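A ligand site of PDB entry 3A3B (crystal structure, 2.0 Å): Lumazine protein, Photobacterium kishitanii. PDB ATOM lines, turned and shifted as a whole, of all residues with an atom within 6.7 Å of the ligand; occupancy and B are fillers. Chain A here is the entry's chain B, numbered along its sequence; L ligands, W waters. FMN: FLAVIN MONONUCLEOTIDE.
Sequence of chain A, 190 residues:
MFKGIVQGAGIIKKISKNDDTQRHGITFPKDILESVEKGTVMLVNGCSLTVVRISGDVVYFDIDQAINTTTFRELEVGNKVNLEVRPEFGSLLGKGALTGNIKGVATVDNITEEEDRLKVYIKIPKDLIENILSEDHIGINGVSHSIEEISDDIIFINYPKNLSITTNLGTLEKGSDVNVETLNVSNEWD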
ATOM      1  N   VAL A  41      -1.986   4.721   3.118  1.00  0.00           N
ATOM      2  CA  VAL A  41      -0.810   4.196   2.440  1.00  0.00           C
ATOM      3  C   VAL A  41      -0.983   2.685   2.302  1.00  0.00           C
ATOM      4  O   VAL A  41      -1.089   1.988   3.310  1.00  0.00           O
ATOM      5  CB  VAL A  41       0.470   4.502   3.218  1.00  0.00           C
ATOM      6  CG1 VAL A  41       1.641   3.926   2.509  1.00  0.00           C
ATOM      7  CG2 VAL A  41       0.596   6.052   3.429  1.00  0.00           C
ATOM      8  N   MET A  42      -1.051   2.191   1.070  1.00  0.00           N
ATOM      9  CA  MET A  42      -1.341   0.757   0.863  1.00  0.00           C
ATOM     10  C   MET A  42      -0.451   0.224  -0.250  1.00  0.00           C
ATOM     11  O   MET A  42       0.293   0.990  -0.835  1.00  0.00           O
ATOM     12  CB  MET A  42      -2.829   0.588   0.535  1.00  0.00           C
ATOM     13  CG  MET A  42      -3.243   1.249  -0.769  1.00  0.00           C
ATOM     14  SD  MET A  42      -4.951   0.912  -1.123  1.00  0.00           S
ATOM     15  CE  MET A  42      -4.923  -0.855  -1.508  1.00  0.00           C
ATOM     16  N   GLY A  46       2.487  -4.189  -5.089  1.00  0.00           N
ATOM     17  CA  GLY A  46       3.586  -4.309  -4.157  1.00  0.00           C
ATOM     18  C   GLY A  46       4.247  -2.966  -3.841  1.00  0.00           C
ATOM     19  O   GLY A  46       5.183  -2.935  -3.076  1.00  0.00           O
ATOM     20  N   CYS A  47       3.754  -1.868  -4.409  1.00  0.00           N
ATOM     21  CA  CYS A  47       4.387  -0.558  -4.201  1.00  0.00           C
ATOM     22  C   CYS A  47       3.576   0.321  -3.210  1.00  0.00           C
ATOM     23  O   CYS A  47       2.342   0.457  -3.367  1.00  0.00           O
ATOM     24  CB  CYS A  47       4.573   0.153  -5.577  1.00  0.00           C
ATOM     25  SG  CYS A  47       5.237   1.855  -5.497  1.00  0.00           S
ATOM     26  N   SER A  48       4.235   0.906  -2.194  1.00  0.00           N
ATOM     27  CA  SER A  48       3.556   1.850  -1.298  1.00  0.00           C
ATOM     28  C   SER A  48       3.190   3.088  -2.058  1.00  0.00           C
ATOM     29  O   SER A  48       4.077   3.792  -2.636  1.00  0.00           O
ATOM     30  CB  SER A  48       4.419   2.271  -0.098  1.00  0.00           C
ATOM     31  OG  SER A  48       4.588   1.176   0.768  1.00  0.00           O
ATOM     32  N   LEU A  49       1.895   3.385  -2.039  1.00  0.00           N
ATOM     33  CA  LEU A  49       1.352   4.577  -2.627  1.00  0.00           C
ATOM     34  C   LEU A  49       0.267   5.103  -1.715  1.00  0.00           C
ATOM     35  O   LEU A  49      -0.408   4.328  -0.996  1.00  0.00           O
ATOM     36  CB  LEU A  49       0.689   4.274  -3.969  1.00  0.00           C
ATOM     37  CG  LEU A  49       1.487   3.686  -5.139  1.00  0.00           C
ATOM     38  CD1 LEU A  49       0.506   3.407  -6.252  1.00  0.00           C
ATOM     39  CD2 LEU A  49       2.563   4.703  -5.579  1.00  0.00           C
ATOM     40  N   THR A  50       0.042   6.406  -1.810  1.00  0.00           N
ATOM     41  CA  THR A  50      -0.921   7.115  -0.940  1.00  0.00           C
ATOM     42  C   THR A  50      -2.186   7.482  -1.666  1.00  0.00           C
ATOM     43  O   THR A  50      -2.145   8.094  -2.737  1.00  0.00           O
ATOM     44  CB  THR A  50      -0.251   8.408  -0.402  1.00  0.00           C
ATOM     45  OG1 THR A  50       1.016   8.067   0.155  1.00  0.00           O
ATOM     46  CG2 THR A  50      -1.109   9.070   0.643  1.00  0.00           C
ATOM     47  N   VAL A  51      -3.337   7.111  -1.066  1.00  0.00           N
ATOM     48  CA  VAL A  51      -4.610   7.475  -1.653  1.00  0.00           C
ATOM     49  C   VAL A  51      -4.789   9.015  -1.623  1.00  0.00           C
ATOM     50  O   VAL A  51      -4.781   9.639  -0.543  1.00  0.00           O
ATOM     51  CB  VAL A  51      -5.783   6.804  -0.893  1.00  0.00           C
ATOM     52  CG1 VAL A  51      -7.121   7.249  -1.512  1.00  0.00           C
ATOM     53  CG2 VAL A  51      -5.675   5.231  -0.915  1.00  0.00           C
ATOM     54  N   VAL A  52      -4.945   9.641  -2.782  1.00  0.00           N
ATOM     55  CA  VAL A  52      -5.126  11.109  -2.820  1.00  0.00           C
ATOM     56  C   VAL A  52      -6.592  11.516  -2.960  1.00  0.00           C
ATOM     57  O   VAL A  52      -6.984  12.614  -2.609  1.00  0.00           O
ATOM     58  CB  VAL A  52      -4.249  11.771  -3.942  1.00  0.00           C
ATOM     59  CG1 VAL A  52      -2.834  11.342  -3.758  1.00  0.00           C
ATOM     60  CG2 VAL A  52      -4.713  11.361  -5.300  1.00  0.00           C
ATOM     61  N   PHE A  61      -4.375   7.578  -7.073  1.00  0.00           N
ATOM     62  CA  PHE A  61      -3.008   7.630  -6.513  1.00  0.00           C
ATOM     63  C   PHE A  61      -2.234   8.495  -7.484  1.00  0.00           C
ATOM     64  O   PHE A  61      -2.507   8.460  -8.632  1.00  0.00           O
ATOM     65  CB  PHE A  61      -2.406   6.219  -6.551  1.00  0.00           C
ATOM     66  CG  PHE A  61      -3.121   5.241  -5.694  1.00  0.00           C
ATOM     67  CD1 PHE A  61      -2.754   5.092  -4.336  1.00  0.00           C
ATOM     68  CD2 PHE A  61      -4.156   4.446  -6.232  1.00  0.00           C
ATOM     69  CE1 PHE A  61      -3.422   4.167  -3.489  1.00  0.00           C
ATOM     70  CE2 PHE A  61      -4.847   3.521  -5.413  1.00  0.00           C
ATOM     71  CZ  PHE A  61      -4.474   3.386  -4.047  1.00  0.00           C
ATOM     72  N   ASP A  62      -1.310   9.297  -7.005  1.00  0.00           N
ATOM     73  CA  ASP A  62      -0.403  10.037  -7.900  1.00  0.00           C
ATOM     74  C   ASP A  62       0.903   9.284  -7.946  1.00  0.00           C
ATOM     75  O   ASP A  62       1.484   9.022  -6.923  1.00  0.00           O
ATOM     76  CB  ASP A  62      -0.124  11.456  -7.379  1.00  0.00           C
ATOM     77  CG  ASP A  62      -1.269  12.412  -7.640  1.00  0.00           C
ATOM     78  OD1 ASP A  62      -1.852  12.401  -8.742  1.00  0.00           O
ATOM     79  OD2 ASP A  62      -1.572  13.186  -6.730  1.00  0.00           O
ATOM     80  N   ILE A  63       1.329   8.900  -9.126  1.00  0.00           N
ATOM     81  CA  ILE A  63       2.610   8.203  -9.226  1.00  0.00           C
ATOM     82  C   ILE A  63       3.593   9.259  -9.652  1.00  0.00           C
ATOM     83  O   ILE A  63       3.527   9.757 -10.769  1.00  0.00           O
ATOM     84  CB  ILE A  63       2.631   7.082 -10.338  1.00  0.00           C
ATOM     85  CG1 ILE A  63       1.375   6.172 -10.320  1.00  0.00           C
ATOM     86  CG2 ILE A  63       3.972   6.293 -10.266  1.00  0.00           C
ATOM     87  CD1 ILE A  63       1.105   5.574  -9.001  1.00  0.00           C
ATOM     88  N   ASP A  64       4.488   9.606  -8.757  1.00  0.00           N
ATOM     89  CA  ASP A  64       5.487  10.613  -9.067  1.00  0.00           C
ATOM     90  C   ASP A  64       6.857  10.151  -8.553  1.00  0.00           C
ATOM     91  O   ASP A  64       7.695   9.818  -9.357  1.00  0.00           O
ATOM     92  CB  ASP A  64       5.067  11.999  -8.542  1.00  0.00           C
ATOM     93  CG  ASP A  64       4.323  11.924  -7.221  1.00  0.00           C
ATOM     94  OD1 ASP A  64       4.690  11.087  -6.372  1.00  0.00           O
ATOM     95  OD2 ASP A  64       3.347  12.701  -7.056  1.00  0.00           O
ATOM     96  N   GLN A  65       7.054  10.086  -7.229  1.00  0.00           N
ATOM     97  CA  GLN A  65       8.256   9.479  -6.675  1.00  0.00           C
ATOM     98  C   GLN A  65       8.587   8.074  -7.212  1.00  0.00           C
ATOM     99  O   GLN A  65       9.761   7.737  -7.378  1.00  0.00           O
ATOM    100  CB  GLN A  65       8.136   9.417  -5.159  1.00  0.00           C
ATOM    101  CG  GLN A  65       9.297   8.744  -4.460  1.00  0.00           C
ATOM    102  CD  GLN A  65       9.176   8.775  -2.948  1.00  0.00           C
ATOM    103  OE1 GLN A  65       8.132   9.164  -2.376  1.00  0.00           O
ATOM    104  NE2 GLN A  65      10.254   8.370  -2.281  1.00  0.00           N
ATOM    105  N   ALA A  66       7.566   7.270  -7.494  1.00  0.00           N
ATOM    106  CA  ALA A  66       7.773   5.876  -7.965  1.00  0.00           C
ATOM    107  C   ALA A  66       7.878   5.740  -9.476  1.00  0.00           C
ATOM    108  O   ALA A  66       8.101   4.642 -10.010  1.00  0.00           O
ATOM    109  CB  ALA A  66       6.620   4.969  -7.417  1.00  0.00           C
ATOM    110  N   ILE A  67       7.685   6.856 -10.192  1.00  0.00           N
ATOM    111  CA  ILE A  67       7.399   6.819 -11.670  1.00  0.00           C
ATOM    112  C   ILE A  67       8.493   6.185 -12.561  1.00  0.00           C
ATOM    113  O   ILE A  67       8.200   5.639 -13.633  1.00  0.00           O
ATOM    114  CB  ILE A  67       7.014   8.221 -12.220  1.00  0.00           C
ATOM    115  CG1 ILE A  67       6.284   8.173 -13.564  1.00  0.00           C
ATOM    116  CG2 ILE A  67       8.265   9.080 -12.378  1.00  0.00           C
ATOM    117  CD1 ILE A  67       4.795   7.835 -13.534  1.00  0.00           C
ATOM    118  N   ASN A  68       9.737   6.254 -12.131  1.00  0.00           N
ATOM    119  CA  ASN A  68      10.857   5.763 -12.965  1.00  0.00           C
ATOM    120  C   ASN A  68      11.411   4.414 -12.560  1.00  0.00           C
ATOM    121  O   ASN A  68      12.283   3.890 -13.237  1.00  0.00           O
ATOM    122  CB  ASN A  68      12.011   6.793 -13.016  1.00  0.00           C
ATOM    123  CG  ASN A  68      11.564   8.117 -13.565  1.00  0.00           C
ATOM    124  OD1 ASN A  68      11.794   9.158 -12.937  1.00  0.00           O
ATOM    125  ND2 ASN A  68      10.887   8.091 -14.736  1.00  0.00           N
ATOM    126  N   THR A  69      10.864   3.858 -11.470  1.00  0.00           N
ATOM    127  CA  THR A  69      11.373   2.648 -10.790  1.00  0.00           C
ATOM    128  C   THR A  69      10.273   1.613 -10.516  1.00  0.00           C
ATOM    129  O   THR A  69      10.450   0.730  -9.639  1.00  0.00           O
ATOM    130  CB  THR A  69      11.960   3.059  -9.458  1.00  0.00           C
ATOM    131  OG1 THR A  69      11.028   3.942  -8.788  1.00  0.00           O
ATOM    132  CG2 THR A  69      13.322   3.799  -9.690  1.00  0.00           C
ATOM    133  N   THR A  70       9.156   1.740 -11.239  1.00  0.00           N
ATOM    134  CA  THR A  70       8.007   0.826 -11.077  1.00  0.00           C
ATOM    135  C   THR A  70       7.391   0.694 -12.449  1.00  0.00           C
ATOM    136  O   THR A  70       7.745   1.419 -13.343  1.00  0.00           O
ATOM    137  CB  THR A  70       6.970   1.296 -10.005  1.00  0.00           C
ATOM    138  OG1 THR A  70       6.437   2.574 -10.375  1.00  0.00           O
ATOM    139  CG2 THR A  70       7.568   1.371  -8.613  1.00  0.00           C
ATOM    140  N   THR A  99       7.879  -4.400   2.499  1.00  0.00           N
ATOM    141  CA  THR A  99       7.894  -3.014   2.891  1.00  0.00           C
ATOM    142  C   THR A  99       7.175  -2.092   1.909  1.00  0.00           C
ATOM    143  O   THR A  99       6.758  -0.984   2.303  1.00  0.00           O
ATOM    144  CB  THR A  99       9.328  -2.510   3.125  1.00  0.00           C
ATOM    145  OG1 THR A  99       9.991  -2.341   1.861  1.00  0.00           O
ATOM    146  CG2 THR A  99      10.128  -3.481   3.994  1.00  0.00           C
ATOM    147  N   GLY A 100       7.032  -2.507   0.643  1.00  0.00           N
ATOM    148  CA  GLY A 100       6.425  -1.632  -0.346  1.00  0.00           C
ATOM    149  C   GLY A 100       7.411  -0.727  -1.044  1.00  0.00           C
ATOM    150  O   GLY A 100       7.026   0.117  -1.868  1.00  0.00           O
ATOM    151  N   ASN A 101       8.696  -0.939  -0.732  1.00  0.00           N
ATOM    152  CA  ASN A 101       9.805  -0.271  -1.447  1.00  0.00           C
ATOM    153  C   ASN A 101      10.251  -1.192  -2.575  1.00  0.00           C
ATOM    154  O   ASN A 101      10.925  -2.184  -2.334  1.00  0.00           O
ATOM    155  CB  ASN A 101      10.978   0.042  -0.477  1.00  0.00           C
ATOM    156  CG  ASN A 101      12.056   0.900  -1.144  1.00  0.00           C
ATOM    157  OD1 ASN A 101      11.759   1.975  -1.655  1.00  0.00           O
ATOM    158  ND2 ASN A 101      13.285   0.411  -1.165  1.00  0.00           N
ATOM    159  N   ILE A 102       9.828  -0.896  -3.806  1.00  0.00           N
ATOM    160  CA  ILE A 102      10.154  -1.709  -4.968  1.00  0.00           C
ATOM    161  C   ILE A 102      11.633  -1.512  -5.266  1.00  0.00           C
ATOM    162  O   ILE A 102      12.082  -0.383  -5.393  1.00  0.00           O
ATOM    163  CB  ILE A 102       9.334  -1.319  -6.219  1.00  0.00           C
ATOM    164  CG1 ILE A 102       7.809  -1.636  -6.034  1.00  0.00           C
ATOM    165  CG2 ILE A 102       9.863  -2.025  -7.487  1.00  0.00           C
ATOM    166  CD1 ILE A 102       7.480  -2.967  -5.479  1.00  0.00           C
ATOM    167  N   LYS A 103      12.348  -2.632  -5.444  1.00  0.00           N
ATOM    168  CA  LYS A 103      13.792  -2.633  -5.625  1.00  0.00           C
ATOM    169  C   LYS A 103      14.215  -2.690  -7.078  1.00  0.00           C
ATOM    170  O   LYS A 103      15.340  -2.276  -7.417  1.00  0.00           O
ATOM    171  CB  LYS A 103      14.376  -3.811  -4.887  1.00  0.00           C
ATOM    172  CG  LYS A 103      14.031  -3.826  -3.412  1.00  0.00           C
ATOM    173  CD  LYS A 103      14.556  -2.615  -2.617  1.00  0.00           C
ATOM    174  CE  LYS A 103      14.419  -2.944  -1.122  1.00  0.00           C
ATOM    175  NZ  LYS A 103      14.327  -1.722  -0.222  1.00  0.00           N
HETATM  176  N1  FMN L   1       5.448   7.053  -4.437  1.00  0.00           N
HETATM  177  C2  FMN L   1       4.633   7.615  -5.344  1.00  0.00           C
HETATM  178  O2  FMN L   1       5.017   7.748  -6.491  1.00  0.00           O
HETATM  179  N3  FMN L   1       3.384   8.052  -4.958  1.00  0.00           N
HETATM  180  C4  FMN L   1       2.947   7.882  -3.676  1.00  0.00           C
HETATM  181  O4  FMN L   1       1.743   8.033  -3.459  1.00  0.00           O
HETATM  182  C4A FMN L   1       3.798   7.299  -2.742  1.00  0.00           C
HETATM  183  N5  FMN L   1       3.455   7.135  -1.421  1.00  0.00           N
HETATM  184  C5A FMN L   1       4.359   6.526  -0.550  1.00  0.00           C
HETATM  185  C6  FMN L   1       4.012   6.375   0.777  1.00  0.00           C
HETATM  186  C7  FMN L   1       4.847   5.805   1.724  1.00  0.00           C
HETATM  187  C7M FMN L   1       4.539   5.978   3.193  1.00  0.00           C
HETATM  188  C8  FMN L   1       6.105   5.380   1.305  1.00  0.00           C
HETATM  189  C8M FMN L   1       7.077   4.854   2.339  1.00  0.00           C
HETATM  190  C9  FMN L   1       6.498   5.539  -0.041  1.00  0.00           C
HETATM  191  C9A FMN L   1       5.609   6.107  -0.984  1.00  0.00           C
HETATM  192  N10 FMN L   1       5.964   6.307  -2.289  1.00  0.00           N
HETATM  193  C10 FMN L   1       5.071   6.888  -3.149  1.00  0.00           C
HETATM  194  C1' FMN L   1       7.311   5.891  -2.844  1.00  0.00           C
HETATM  195  C2' FMN L   1       7.264   4.509  -3.540  1.00  0.00           C
HETATM  196  O2' FMN L   1       6.865   3.512  -2.642  1.00  0.00           O
HETATM  197  C3' FMN L   1       8.690   4.220  -3.996  1.00  0.00           C
HETATM  198  O3' FMN L   1       9.053   5.266  -4.864  1.00  0.00           O
HETATM  199  C4' FMN L   1       8.908   2.861  -4.711  1.00  0.00           C
HETATM  200  O4' FMN L   1       8.427   1.792  -3.971  1.00  0.00           O
HETATM  201  C5' FMN L   1      10.338   2.429  -4.467  1.00  0.00           C
HETATM  202  O5' FMN L   1      11.111   2.921  -5.469  1.00  0.00           O
HETATM  203  P   FMN L   1      12.308   4.001  -5.172  1.00  0.00           P
HETATM  204  O1P FMN L   1      13.014   3.852  -6.500  1.00  0.00           O
HETATM  205  O2P FMN L   1      13.187   3.708  -3.960  1.00  0.00           O
HETATM  206  O3P FMN L   1      11.676   5.365  -5.001  1.00  0.00           O
HETATM  207  O   HOH W   1       5.024  10.190  -2.173  1.00  0.00           O
HETATM  208  O   HOH W   2      -0.396   9.043  -4.396  1.00  0.00           O
HETATM  209  O   HOH W   3       8.572   2.898  -0.811  1.00  0.00           O
HETATM  210  O   HOH W   4       7.581   1.586   1.812  1.00  0.00           O
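Water W2 lies within hydrogen-bond range of an oxygen (O4) of the ligand (2.5 Å), the backbone carbonyl oxygen (O) of Thr 50 (2.6 Å) and the backbone NH (N) of Asp 62 (2.8 Å). Water W3 lies within hydrogen-bond range of an oxygen (O2') of the ligand (2.6 Å), the backbone carbonyl oxygen (O) of Gly 100 (3.4 Å) and the side-chain amide oxygen (OD1) of Asn 101 (3.4 Å). Water W4 lies within hydrogen-bond range of O of Thr 99 (2.7 Å) and OG of Ser 48 (3.2 Å).
Val 41 touches the ligand. Leu 49 touches the ligand. Ile 63 touches the ligand (CA to O2, 3.7 Å). 14 residues have an atom within 4 Å of the ligand: Val 41, Cys 47, Ser 48, Leu 49, Thr 50, Asp 62, Ile 63, Asp 64, Gln 65, Ala 66, Thr 69, Gly 100, Asn 101 and Ile 102.
The backbone carbonyl oxygen (O) of Ala 66 sits at hydrogen-bond distance from the side-chain hydroxyl (OG1) of Thr 69 (3.2 Å). The backbone carbonyl oxygen (O) of Ala 66 lies within hydrogen-bond range of the side-chain hydroxyl (OG1) of Thr 70. N of Ser 48 sits at hydrogen-bond distance from O of Gly 100. The side-chain hydroxyl of Ser 48 lies within hydrogen-bond range of the backbone carbonyl oxygen of Thr 99 (3.4 Å). ND2 of Asn 101 sits close to NZ of Lys 103, at 2.6 Å. OG1 of Thr 99 is in hydrogen-bond range of N of Asn 101 (3.2 Å). N of Met 42 is in hydrogen-bond range of O of Leu 49 (3.0 Å).
N of Ala 66 lies within hydrogen-bond range of O2 of the ligand (2.8 Å). An oxygen (O2') of the ligand sits at hydrogen-bond distance from the backbone carbonyl oxygen (O) of Ser 48, 2.8 Å away. O4 of the ligand sits at hydrogen-bond distance from N of Thr 50, 2.9 Å away. OG1 of Thr 50 is in hydrogen-bond range of N5 of the ligand (3.0 Å). A nitrogen (N3) of the ligand is in hydrogen-bond range of the backbone carbonyl oxygen (O) of Asp 62, 2.9 Å away. The backbone NH (N) of Asp 64 sits at hydrogen-bond distance from an oxygen (O2) of the ligand (3.0 Å). O1P of the ligand sits at hydrogen-bond distance from OG1 of Thr 69 (3.0 Å). An oxygen (O4') of the ligand lies within hydrogen-bond range of the backbone carbonyl oxygen of Gly 100, 3.0 Å away. O4' of the ligand is in hydrogen-bond range of N of Ile 102 (3.0 Å). The side-chain amide oxygen (OD1) of Asn 101 sits close to an oxygen (O2P) of the ligand (3.2 Å). O2 of the ligand sits at hydrogen-bond distance from N of Gln 65, at 3.2 Å. An oxygen (O4') of the ligand is in hydrogen-bond range of the side-chain sulfur of Cys 47 (3.5 Å).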
